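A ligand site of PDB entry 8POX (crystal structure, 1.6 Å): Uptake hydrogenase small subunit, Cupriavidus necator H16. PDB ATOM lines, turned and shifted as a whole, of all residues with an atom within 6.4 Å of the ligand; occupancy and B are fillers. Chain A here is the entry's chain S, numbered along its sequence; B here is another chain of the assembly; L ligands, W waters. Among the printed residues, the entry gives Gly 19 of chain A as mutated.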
ATOM      1  N   LEU A  15      -4.455 -17.616  12.158  1.00  0.00           N
ATOM      2  CA  LEU A  15      -5.440 -18.260  11.272  1.00  0.00           C
ATOM      3  C   LEU A  15      -6.075 -17.181  10.416  1.00  0.00           C
ATOM      4  O   LEU A  15      -6.631 -16.210  10.945  1.00  0.00           O
ATOM      5  CB  LEU A  15      -6.517 -18.995  12.066  1.00  0.00           C
ATOM      6  CG  LEU A  15      -6.059 -20.226  12.844  1.00  0.00           C
ATOM      7  CD1 LEU A  15      -7.239 -20.786  13.612  1.00  0.00           C
ATOM      8  CD2 LEU A  15      -5.458 -21.272  11.920  1.00  0.00           C
ATOM      9  N   GLU A  16      -5.999 -17.352   9.103  1.00  0.00           N
ATOM     10  CA  GLU A  16      -6.361 -16.301   8.153  1.00  0.00           C
ATOM     11  C   GLU A  16      -6.510 -16.879   6.760  1.00  0.00           C
ATOM     12  O   GLU A  16      -6.220 -18.060   6.542  1.00  0.00           O
ATOM     13  CB  GLU A  16      -5.285 -15.204   8.140  1.00  0.00           C
ATOM     14  CG  GLU A  16      -3.869 -15.710   8.354  1.00  0.00           C
ATOM     15  CD  GLU A  16      -2.929 -15.528   7.168  1.00  0.00           C
ATOM     16  OE1 GLU A  16      -3.061 -14.552   6.404  1.00  0.00           O
ATOM     17  OE2 GLU A  16      -2.005 -16.347   7.043  1.00  0.00           O
ATOM     18  N   CYS A  17      -6.973 -16.054   5.832  1.00  0.00           N
ATOM     19  CA  CYS A  17      -7.023 -16.427   4.412  1.00  0.00           C
ATOM     20  C   CYS A  17      -6.032 -15.642   3.560  1.00  0.00           C
ATOM     21  O   CYS A  17      -5.921 -15.899   2.362  1.00  0.00           O
ATOM     22  CB  CYS A  17      -8.447 -16.248   3.879  1.00  0.00           C
ATOM     23  SG  CYS A  17      -8.858 -14.594   3.308  1.00  0.00           S
ATOM     24  N   THR A  18      -5.338 -14.677   4.173  1.00  0.00           N
ATOM     25  CA  THR A  18      -4.341 -13.816   3.516  1.00  0.00           C
ATOM     26  C   THR A  18      -4.980 -12.729   2.632  1.00  0.00           C
ATOM     27  O   THR A  18      -4.274 -11.992   1.933  1.00  0.00           O
ATOM     28  CB  THR A  18      -3.278 -14.645   2.765  1.00  0.00           C
ATOM     29  OG1 THR A  18      -2.826 -15.709   3.618  1.00  0.00           O
ATOM     30  CG2 THR A  18      -2.060 -13.799   2.391  1.00  0.00           C
ATOM     31  N   GLY A  19      -6.301 -12.589   2.708  1.00  0.00           N
ATOM     32  CA  GLY A  19      -7.002 -11.538   1.965  1.00  0.00           C
ATOM     33  C   GLY A  19      -6.720 -10.131   2.446  1.00  0.00           C
ATOM     34  O   GLY A  19      -6.856  -9.176   1.676  1.00  0.00           O
ATOM     35  N   CYS A  20      -6.349  -9.977   3.717  1.00  0.00           N
ATOM     36  CA  CYS A  20      -6.013  -8.652   4.249  1.00  0.00           C
ATOM     37  C   CYS A  20      -4.663  -8.166   3.680  1.00  0.00           C
ATOM     38  O   CYS A  20      -4.537  -7.013   3.279  1.00  0.00           O
ATOM     39  CB  CYS A  20      -6.049  -8.630   5.780  1.00  0.00           C
ATOM     40  SG  CYS A  20      -7.710  -8.825   6.504  1.00  0.00           S
ATOM     41  N   SER A  21      -3.671  -9.059   3.621  1.00  0.00           N
ATOM     42  CA  SER A  21      -2.405  -8.776   2.929  1.00  0.00           C
ATOM     43  C   SER A  21      -2.625  -8.404   1.455  1.00  0.00           C
ATOM     44  O   SER A  21      -1.997  -7.471   0.949  1.00  0.00           O
ATOM     45  CB  SER A  21      -1.463  -9.987   2.979  1.00  0.00           C
ATOM     46  OG  SER A  21      -0.783 -10.080   4.209  1.00  0.00           O
ATOM     47  N   GLU A  76      -2.627 -10.034  11.198  1.00  0.00           N
ATOM     48  CA  GLU A  76      -3.609 -10.562  10.278  1.00  0.00           C
ATOM     49  C   GLU A  76      -3.974 -11.954  10.777  1.00  0.00           C
ATOM     50  O   GLU A  76      -3.111 -12.727  11.179  1.00  0.00           O
ATOM     51  CB  GLU A  76      -3.004 -10.622   8.868  1.00  0.00           C
ATOM     52  CG  GLU A  76      -3.899 -11.218   7.798  1.00  0.00           C
ATOM     53  CD  GLU A  76      -3.346 -10.993   6.411  1.00  0.00           C
ATOM     54  OE1 GLU A  76      -2.206 -10.489   6.282  1.00  0.00           O
ATOM     55  OE2 GLU A  76      -4.045 -11.307   5.430  1.00  0.00           O
ATOM     56  N   GLY A  77      -5.265 -12.251  10.813  1.00  0.00           N
ATOM     57  CA  GLY A  77      -5.725 -13.514  11.341  1.00  0.00           C
ATOM     58  C   GLY A  77      -5.861 -13.474  12.853  1.00  0.00           C
ATOM     59  O   GLY A  77      -5.829 -12.402  13.461  1.00  0.00           O
ATOM     60  N   TRP A 112      -5.716  -6.175  11.870  1.00  0.00           N
ATOM     61  CA  TRP A 112      -6.207  -6.109  10.482  1.00  0.00           C
ATOM     62  C   TRP A 112      -7.428  -6.993  10.312  1.00  0.00           C
ATOM     63  O   TRP A 112      -7.401  -8.175  10.645  1.00  0.00           O
ATOM     64  CB  TRP A 112      -5.164  -6.622   9.488  1.00  0.00           C
ATOM     65  CG  TRP A 112      -3.958  -5.775   9.199  1.00  0.00           C
ATOM     66  CD1 TRP A 112      -2.675  -6.211   9.096  1.00  0.00           C
ATOM     67  CD2 TRP A 112      -3.921  -4.374   8.905  1.00  0.00           C
ATOM     68  NE1 TRP A 112      -1.837  -5.177   8.771  1.00  0.00           N
ATOM     69  CE2 TRP A 112      -2.581  -4.032   8.648  1.00  0.00           C
ATOM     70  CE3 TRP A 112      -4.898  -3.367   8.846  1.00  0.00           C
ATOM     71  CZ2 TRP A 112      -2.184  -2.738   8.340  1.00  0.00           C
ATOM     72  CZ3 TRP A 112      -4.495  -2.079   8.543  1.00  0.00           C
ATOM     73  CH2 TRP A 112      -3.153  -1.773   8.296  1.00  0.00           C
ATOM     74  N   GLY A 113      -8.473  -6.418   9.725  1.00  0.00           N
ATOM     75  CA  GLY A 113      -9.620  -7.179   9.260  1.00  0.00           C
ATOM     76  C   GLY A 113     -10.506  -7.763  10.336  1.00  0.00           C
ATOM     77  O   GLY A 113     -10.221  -7.644  11.536  1.00  0.00           O
ATOM     78  N   SER A 114     -11.590  -8.397   9.907  1.00  0.00           N
ATOM     79  CA  SER A 114     -12.523  -9.015  10.840  1.00  0.00           C
ATOM     80  C   SER A 114     -11.948 -10.217  11.594  1.00  0.00           C
ATOM     81  O   SER A 114     -12.379 -10.514  12.711  1.00  0.00           O
ATOM     82  CB  SER A 114     -13.828  -9.355  10.116  1.00  0.00           C
ATOM     83  OG  SER A 114     -14.454  -8.141   9.716  1.00  0.00           O
ATOM     84  N   CYS A 115     -10.949 -10.906  11.024  1.00  0.00           N
ATOM     85  CA  CYS A 115     -10.286 -11.990  11.768  1.00  0.00           C
ATOM     86  C   CYS A 115      -9.651 -11.492  13.062  1.00  0.00           C
ATOM     87  O   CYS A 115      -9.971 -11.975  14.157  1.00  0.00           O
ATOM     88  CB  CYS A 115      -9.209 -12.671  10.928  1.00  0.00           C
ATOM     89  SG  CYS A 115      -9.814 -13.845   9.707  1.00  0.00           S
ATOM     90  N   ALA A 116      -8.738 -10.538  12.944  1.00  0.00           N
ATOM     91  CA  ALA A 116      -8.023 -10.025  14.109  1.00  0.00           C
ATOM     92  C   ALA A 116      -8.946  -9.222  15.014  1.00  0.00           C
ATOM     93  O   ALA A 116      -8.797  -9.263  16.227  1.00  0.00           O
ATOM     94  CB  ALA A 116      -6.837  -9.180  13.666  1.00  0.00           C
ATOM     95  N   CYS A 120     -14.126 -13.588  12.767  1.00  0.00           N
ATOM     96  CA  CYS A 120     -14.444 -13.865  11.375  1.00  0.00           C
ATOM     97  C   CYS A 120     -14.827 -15.338  11.133  1.00  0.00           C
ATOM     98  O   CYS A 120     -15.423 -15.964  12.006  1.00  0.00           O
ATOM     99  CB  CYS A 120     -13.328 -13.376  10.454  1.00  0.00           C
ATOM    100  SG  CYS A 120     -13.908 -12.950   8.781  1.00  0.00           S
ATOM    101  N   VAL A 121     -14.535 -15.874   9.949  1.00  0.00           N
ATOM    102  CA  VAL A 121     -15.212 -17.079   9.492  1.00  0.00           C
ATOM    103  C   VAL A 121     -14.879 -18.301  10.361  1.00  0.00           C
ATOM    104  O   VAL A 121     -15.764 -19.084  10.695  1.00  0.00           O
ATOM    105  CB  VAL A 121     -14.964 -17.334   7.981  1.00  0.00           C
ATOM    106  CG1 VAL A 121     -13.561 -17.854   7.702  1.00  0.00           C
ATOM    107  CG2 VAL A 121     -16.015 -18.287   7.438  1.00  0.00           C
ATOM    108  N   GLN A 122     -13.629 -18.429  10.755  1.00  0.00           N
ATOM    109  CA  GLN A 122     -13.214 -19.554  11.592  1.00  0.00           C
ATOM    110  C   GLN A 122     -13.851 -19.511  12.996  1.00  0.00           C
ATOM    111  O   GLN A 122     -13.959 -20.546  13.638  1.00  0.00           O
ATOM    112  CB  GLN A 122     -11.691 -19.637  11.710  1.00  0.00           C
ATOM    113  CG  GLN A 122     -11.011 -18.384  12.233  1.00  0.00           C
ATOM    114  CD  GLN A 122     -10.538 -17.470  11.128  1.00  0.00           C
ATOM    115  OE1 GLN A 122     -11.169 -17.359  10.083  1.00  0.00           O
ATOM    116  NE2 GLN A 122      -9.413 -16.800  11.354  1.00  0.00           N
ATOM    117  N   GLY A 148     -13.427  -5.603   8.513  1.00  0.00           N
ATOM    118  CA  GLY A 148     -13.791  -5.785   7.122  1.00  0.00           C
ATOM    119  C   GLY A 148     -13.139  -7.054   6.648  1.00  0.00           C
ATOM    120  O   GLY A 148     -12.082  -7.461   7.176  1.00  0.00           O
ATOM    121  N   CYS A 149     -13.739  -7.697   5.650  1.00  0.00           N
ATOM    122  CA  CYS A 149     -13.279  -8.997   5.186  1.00  0.00           C
ATOM    123  C   CYS A 149     -13.052  -9.004   3.668  1.00  0.00           C
ATOM    124  O   CYS A 149     -13.915  -9.482   2.907  1.00  0.00           O
ATOM    125  CB  CYS A 149     -14.266 -10.074   5.600  1.00  0.00           C
ATOM    126  SG  CYS A 149     -13.633 -11.758   5.427  1.00  0.00           S
ATOM    127  N   PRO A 150     -11.921  -8.442   3.212  1.00  0.00           N
ATOM    128  CA  PRO A 150     -10.932  -7.671   3.971  1.00  0.00           C
ATOM    129  C   PRO A 150     -11.362  -6.208   4.078  1.00  0.00           C
ATOM    130  O   PRO A 150     -12.347  -5.832   3.475  1.00  0.00           O
ATOM    131  CB  PRO A 150      -9.688  -7.760   3.092  1.00  0.00           C
ATOM    132  CG  PRO A 150     -10.222  -7.827   1.698  1.00  0.00           C
ATOM    133  CD  PRO A 150     -11.592  -8.456   1.773  1.00  0.00           C
ATOM    134  N   PRO A 151     -10.626  -5.389   4.845  1.00  0.00           N
ATOM    135  CA  PRO A 151     -10.876  -3.954   4.783  1.00  0.00           C
ATOM    136  C   PRO A 151     -10.528  -3.391   3.412  1.00  0.00           C
ATOM    137  O   PRO A 151      -9.754  -4.006   2.674  1.00  0.00           O
ATOM    138  CB  PRO A 151      -9.938  -3.360   5.838  1.00  0.00           C
ATOM    139  CG  PRO A 151      -9.427  -4.514   6.636  1.00  0.00           C
ATOM    140  CD  PRO A 151      -9.499  -5.712   5.738  1.00  0.00           C
ATOM    141  N   TRP A 258     -21.248 -13.743  10.402  1.00  0.00           N
ATOM    142  CA  TRP A 258     -21.551 -15.063   9.833  1.00  0.00           C
ATOM    143  C   TRP A 258     -22.713 -15.768  10.540  1.00  0.00           C
ATOM    144  O   TRP A 258     -23.242 -16.746  10.022  1.00  0.00           O
ATOM    145  CB  TRP A 258     -20.314 -15.953   9.876  1.00  0.00           C
ATOM    146  CG  TRP A 258     -19.109 -15.365   9.204  1.00  0.00           C
ATOM    147  CD1 TRP A 258     -18.088 -14.697   9.812  1.00  0.00           C
ATOM    148  CD2 TRP A 258     -18.797 -15.404   7.815  1.00  0.00           C
ATOM    149  NE1 TRP A 258     -17.164 -14.315   8.876  1.00  0.00           N
ATOM    150  CE2 TRP A 258     -17.568 -14.745   7.641  1.00  0.00           C
ATOM    151  CE3 TRP A 258     -19.425 -15.951   6.684  1.00  0.00           C
ATOM    152  CZ2 TRP A 258     -16.964 -14.586   6.402  1.00  0.00           C
ATOM    153  CZ3 TRP A 258     -18.822 -15.800   5.456  1.00  0.00           C
ATOM    154  CH2 TRP A 258     -17.600 -15.122   5.320  1.00  0.00           C
ATOM    155  N   ARG B  53      -8.744 -24.400  10.204  1.00  0.00           N
ATOM    156  CA  ARG B  53      -9.843 -23.545  10.639  1.00  0.00           C
ATOM    157  C   ARG B  53     -11.181 -24.299  10.751  1.00  0.00           C
ATOM    158  O   ARG B  53     -12.003 -23.959  11.594  1.00  0.00           O
ATOM    159  CB  ARG B  53      -9.971 -22.366   9.678  1.00  0.00           C
ATOM    160  CG  ARG B  53      -8.915 -21.296   9.875  1.00  0.00           C
ATOM    161  CD  ARG B  53      -8.890 -20.276   8.743  1.00  0.00           C
ATOM    162  NE  ARG B  53      -8.575 -20.920   7.481  1.00  0.00           N
ATOM    163  CZ  ARG B  53      -8.893 -20.472   6.272  1.00  0.00           C
ATOM    164  NH1 ARG B  53      -9.510 -19.303   6.104  1.00  0.00           N
ATOM    165  NH2 ARG B  53      -8.572 -21.202   5.207  1.00  0.00           N
ATOM    166  N   ARG B  73     -13.781 -17.452   1.767  1.00  0.00           N
ATOM    167  CA  ARG B  73     -12.836 -17.048   2.799  1.00  0.00           C
ATOM    168  C   ARG B  73     -11.886 -18.162   3.227  1.00  0.00           C
ATOM    169  O   ARG B  73     -11.100 -17.978   4.146  1.00  0.00           O
ATOM    170  CB  ARG B  73     -13.570 -16.473   4.006  1.00  0.00           C
ATOM    171  CG  ARG B  73     -13.843 -14.968   3.921  1.00  0.00           C
ATOM    172  CD  ARG B  73     -14.763 -14.573   2.791  1.00  0.00           C
ATOM    173  NE  ARG B  73     -15.070 -13.145   2.883  1.00  0.00           N
ATOM    174  CZ  ARG B  73     -16.023 -12.499   2.214  1.00  0.00           C
ATOM    175  NH1 ARG B  73     -16.826 -13.144   1.371  1.00  0.00           N
ATOM    176  NH2 ARG B  73     -16.164 -11.191   2.398  1.00  0.00           N
ATOM    177  N   CYS B  75      -9.596 -18.708   1.214  1.00  0.00           N
ATOM    178  CA  CYS B  75      -8.377 -18.111   0.693  1.00  0.00           C
ATOM    179  C   CYS B  75      -8.619 -16.794  -0.023  1.00  0.00           C
ATOM    180  O   CYS B  75      -9.429 -16.710  -0.935  1.00  0.00           O
ATOM    181  CB  CYS B  75      -7.700 -19.076  -0.258  1.00  0.00           C
ATOM    182  SG  CYS B  75      -6.078 -18.501  -0.835  1.00  0.00           S
ATOM    183  N   GLY B  76      -7.874 -15.771   0.387  1.00  0.00           N
ATOM    184  CA  GLY B  76      -7.919 -14.449  -0.228  1.00  0.00           C
ATOM    185  C   GLY B  76      -6.935 -14.243  -1.370  1.00  0.00           C
ATOM    186  O   GLY B  76      -6.952 -13.187  -2.015  1.00  0.00           O
ATOM    187  N   PRO B 228      -9.928  -8.122  -2.721  1.00  0.00           N
ATOM    188  CA  PRO B 228     -10.341  -9.522  -2.636  1.00  0.00           C
ATOM    189  C   PRO B 228     -11.815  -9.791  -2.272  1.00  0.00           C
ATOM    190  O   PRO B 228     -12.522  -8.891  -1.824  1.00  0.00           O
ATOM    191  CB  PRO B 228      -9.438 -10.089  -1.536  1.00  0.00           C
ATOM    192  CG  PRO B 228      -8.267  -9.183  -1.491  1.00  0.00           C
ATOM    193  CD  PRO B 228      -8.800  -7.826  -1.825  1.00  0.00           C
ATOM    194  N   HIS B 229     -12.241 -11.035  -2.518  1.00  0.00           N
ATOM    195  CA  HIS B 229     -13.555 -11.592  -2.147  1.00  0.00           C
ATOM    196  C   HIS B 229     -14.757 -10.965  -2.870  1.00  0.00           C
ATOM    197  O   HIS B 229     -15.684 -10.470  -2.237  1.00  0.00           O
ATOM    198  CB  HIS B 229     -13.741 -11.580  -0.632  1.00  0.00           C
ATOM    199  CG  HIS B 229     -12.760 -12.447   0.097  1.00  0.00           C
ATOM    200  ND1 HIS B 229     -12.182 -13.571  -0.464  1.00  0.00           N
ATOM    201  CD2 HIS B 229     -12.274 -12.373   1.366  1.00  0.00           C
ATOM    202  CE1 HIS B 229     -11.395 -14.148   0.419  1.00  0.00           C
ATOM    203  NE2 HIS B 229     -11.422 -13.435   1.533  1.00  0.00           N
HETATM  204 FE1  LIG L   1      -9.321 -13.244   5.078  1.00  0.00          FE
HETATM  205 FE2  LIG L   1      -9.684 -12.835   7.684  1.00  0.00          FE
HETATM  206 FE3  LIG L   1     -11.388 -11.855   5.812  1.00  0.00          FE
HETATM  207 FE4  LIG L   1      -8.832 -10.766   6.041  1.00  0.00          FE
HETATM  208  S1  LIG L   1     -10.542 -10.702   7.637  1.00  0.00           S
HETATM  209  S2  LIG L   1      -9.965 -11.280   4.161  1.00  0.00           S
HETATM  210  S3  LIG L   1      -7.695 -12.653   6.548  1.00  0.00           S
HETATM  211  S4  LIG L   1     -11.028 -14.082   6.316  1.00  0.00           S
HETATM  212  O   HOH W   1      -9.743 -16.980   7.760  1.00  0.00           O
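The backbone NH (N) of Cys 115 sits close to a sulfur (S1) of the ligand (3.4 Å). An iron atom (FE2) of the ligand is bound by the side-chain sulfur of Cys 115 (2.3 Å). The backbone NH (N) of Cys 17 sits close to a sulfur (S3) of the ligand (3.5 Å). An iron atom (FE1) of the ligand is bound by the side-chain sulfur (SG) of Cys 17 (2.3 Å). The side-chain sulfur of Cys 149 binds an iron atom (FE3) of the ligand (2.3 Å). An iron atom (FE4) of the ligand is bound by the side-chain sulfur of Cys 20 (2.3 Å). S1 of the ligand sits close to N of Ser 114, at 3.4 Å. A ring nitrogen (NE2) of His 229 of chain B lies close to a sulfur (S2) of the ligand, at 3.7 Å.
The side-chain amide nitrogen (NE2) of Gln 122 sits close to the side-chain sulfur (SG) of Cys 115 (3.4 Å). SG of Cys 17 sits close to N of Gly 19 (3.3 Å). The side-chain sulfur (SG) of Cys 17 lies close to a ring nitrogen (NE2) of His 229 of chain B (3.3 Å). N of Gly 76 of chain B sits at hydrogen-bond distance from O of Cys 17, 2.8 Å away. O of Cys 149 sits at hydrogen-bond distance from NH2 of Arg 73 of chain B, 2.9 Å away. SG of Cys 149 sits close to SG of Cys 120, 3.6 Å away. The backbone NH of Ser 114 is in hydrogen-bond range of the backbone carbonyl oxygen of Gly 148 (2.9 Å). The side-chain carboxylate of Glu 16 is in hydrogen-bond range of the side-chain hydroxyl of Thr 18 (3.0 Å).
A sulfur (S1) of the ligand sits close to the backbone carbonyl oxygen (O) of Gly 148 (3.6 Å). A sulfur (S2) of the ligand sits close to the backbone nitrogen (N) of Pro 150 (3.6 Å). CB of Glu 16 touches S3 of the ligand, at 3.9 Å. N of Thr 18 touches S3 of the ligand, at 3.9 Å. CA of Gly 19 touches S2 of the ligand, 3.7 Å away. CA of Gly 113 touches S1 of the ligand, 3.99 Å away. Cys 120 touches the ligand. Arg 73 of chain B touches the ligand.
Water W1 lies within hydrogen-bond range of OE1 of Gln 122 (2.8 Å), NH1 of Arg 53 of chain B (2.9 Å), S4 of the ligand (3.5 Å) and N of Cys 17 (3.5 Å).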
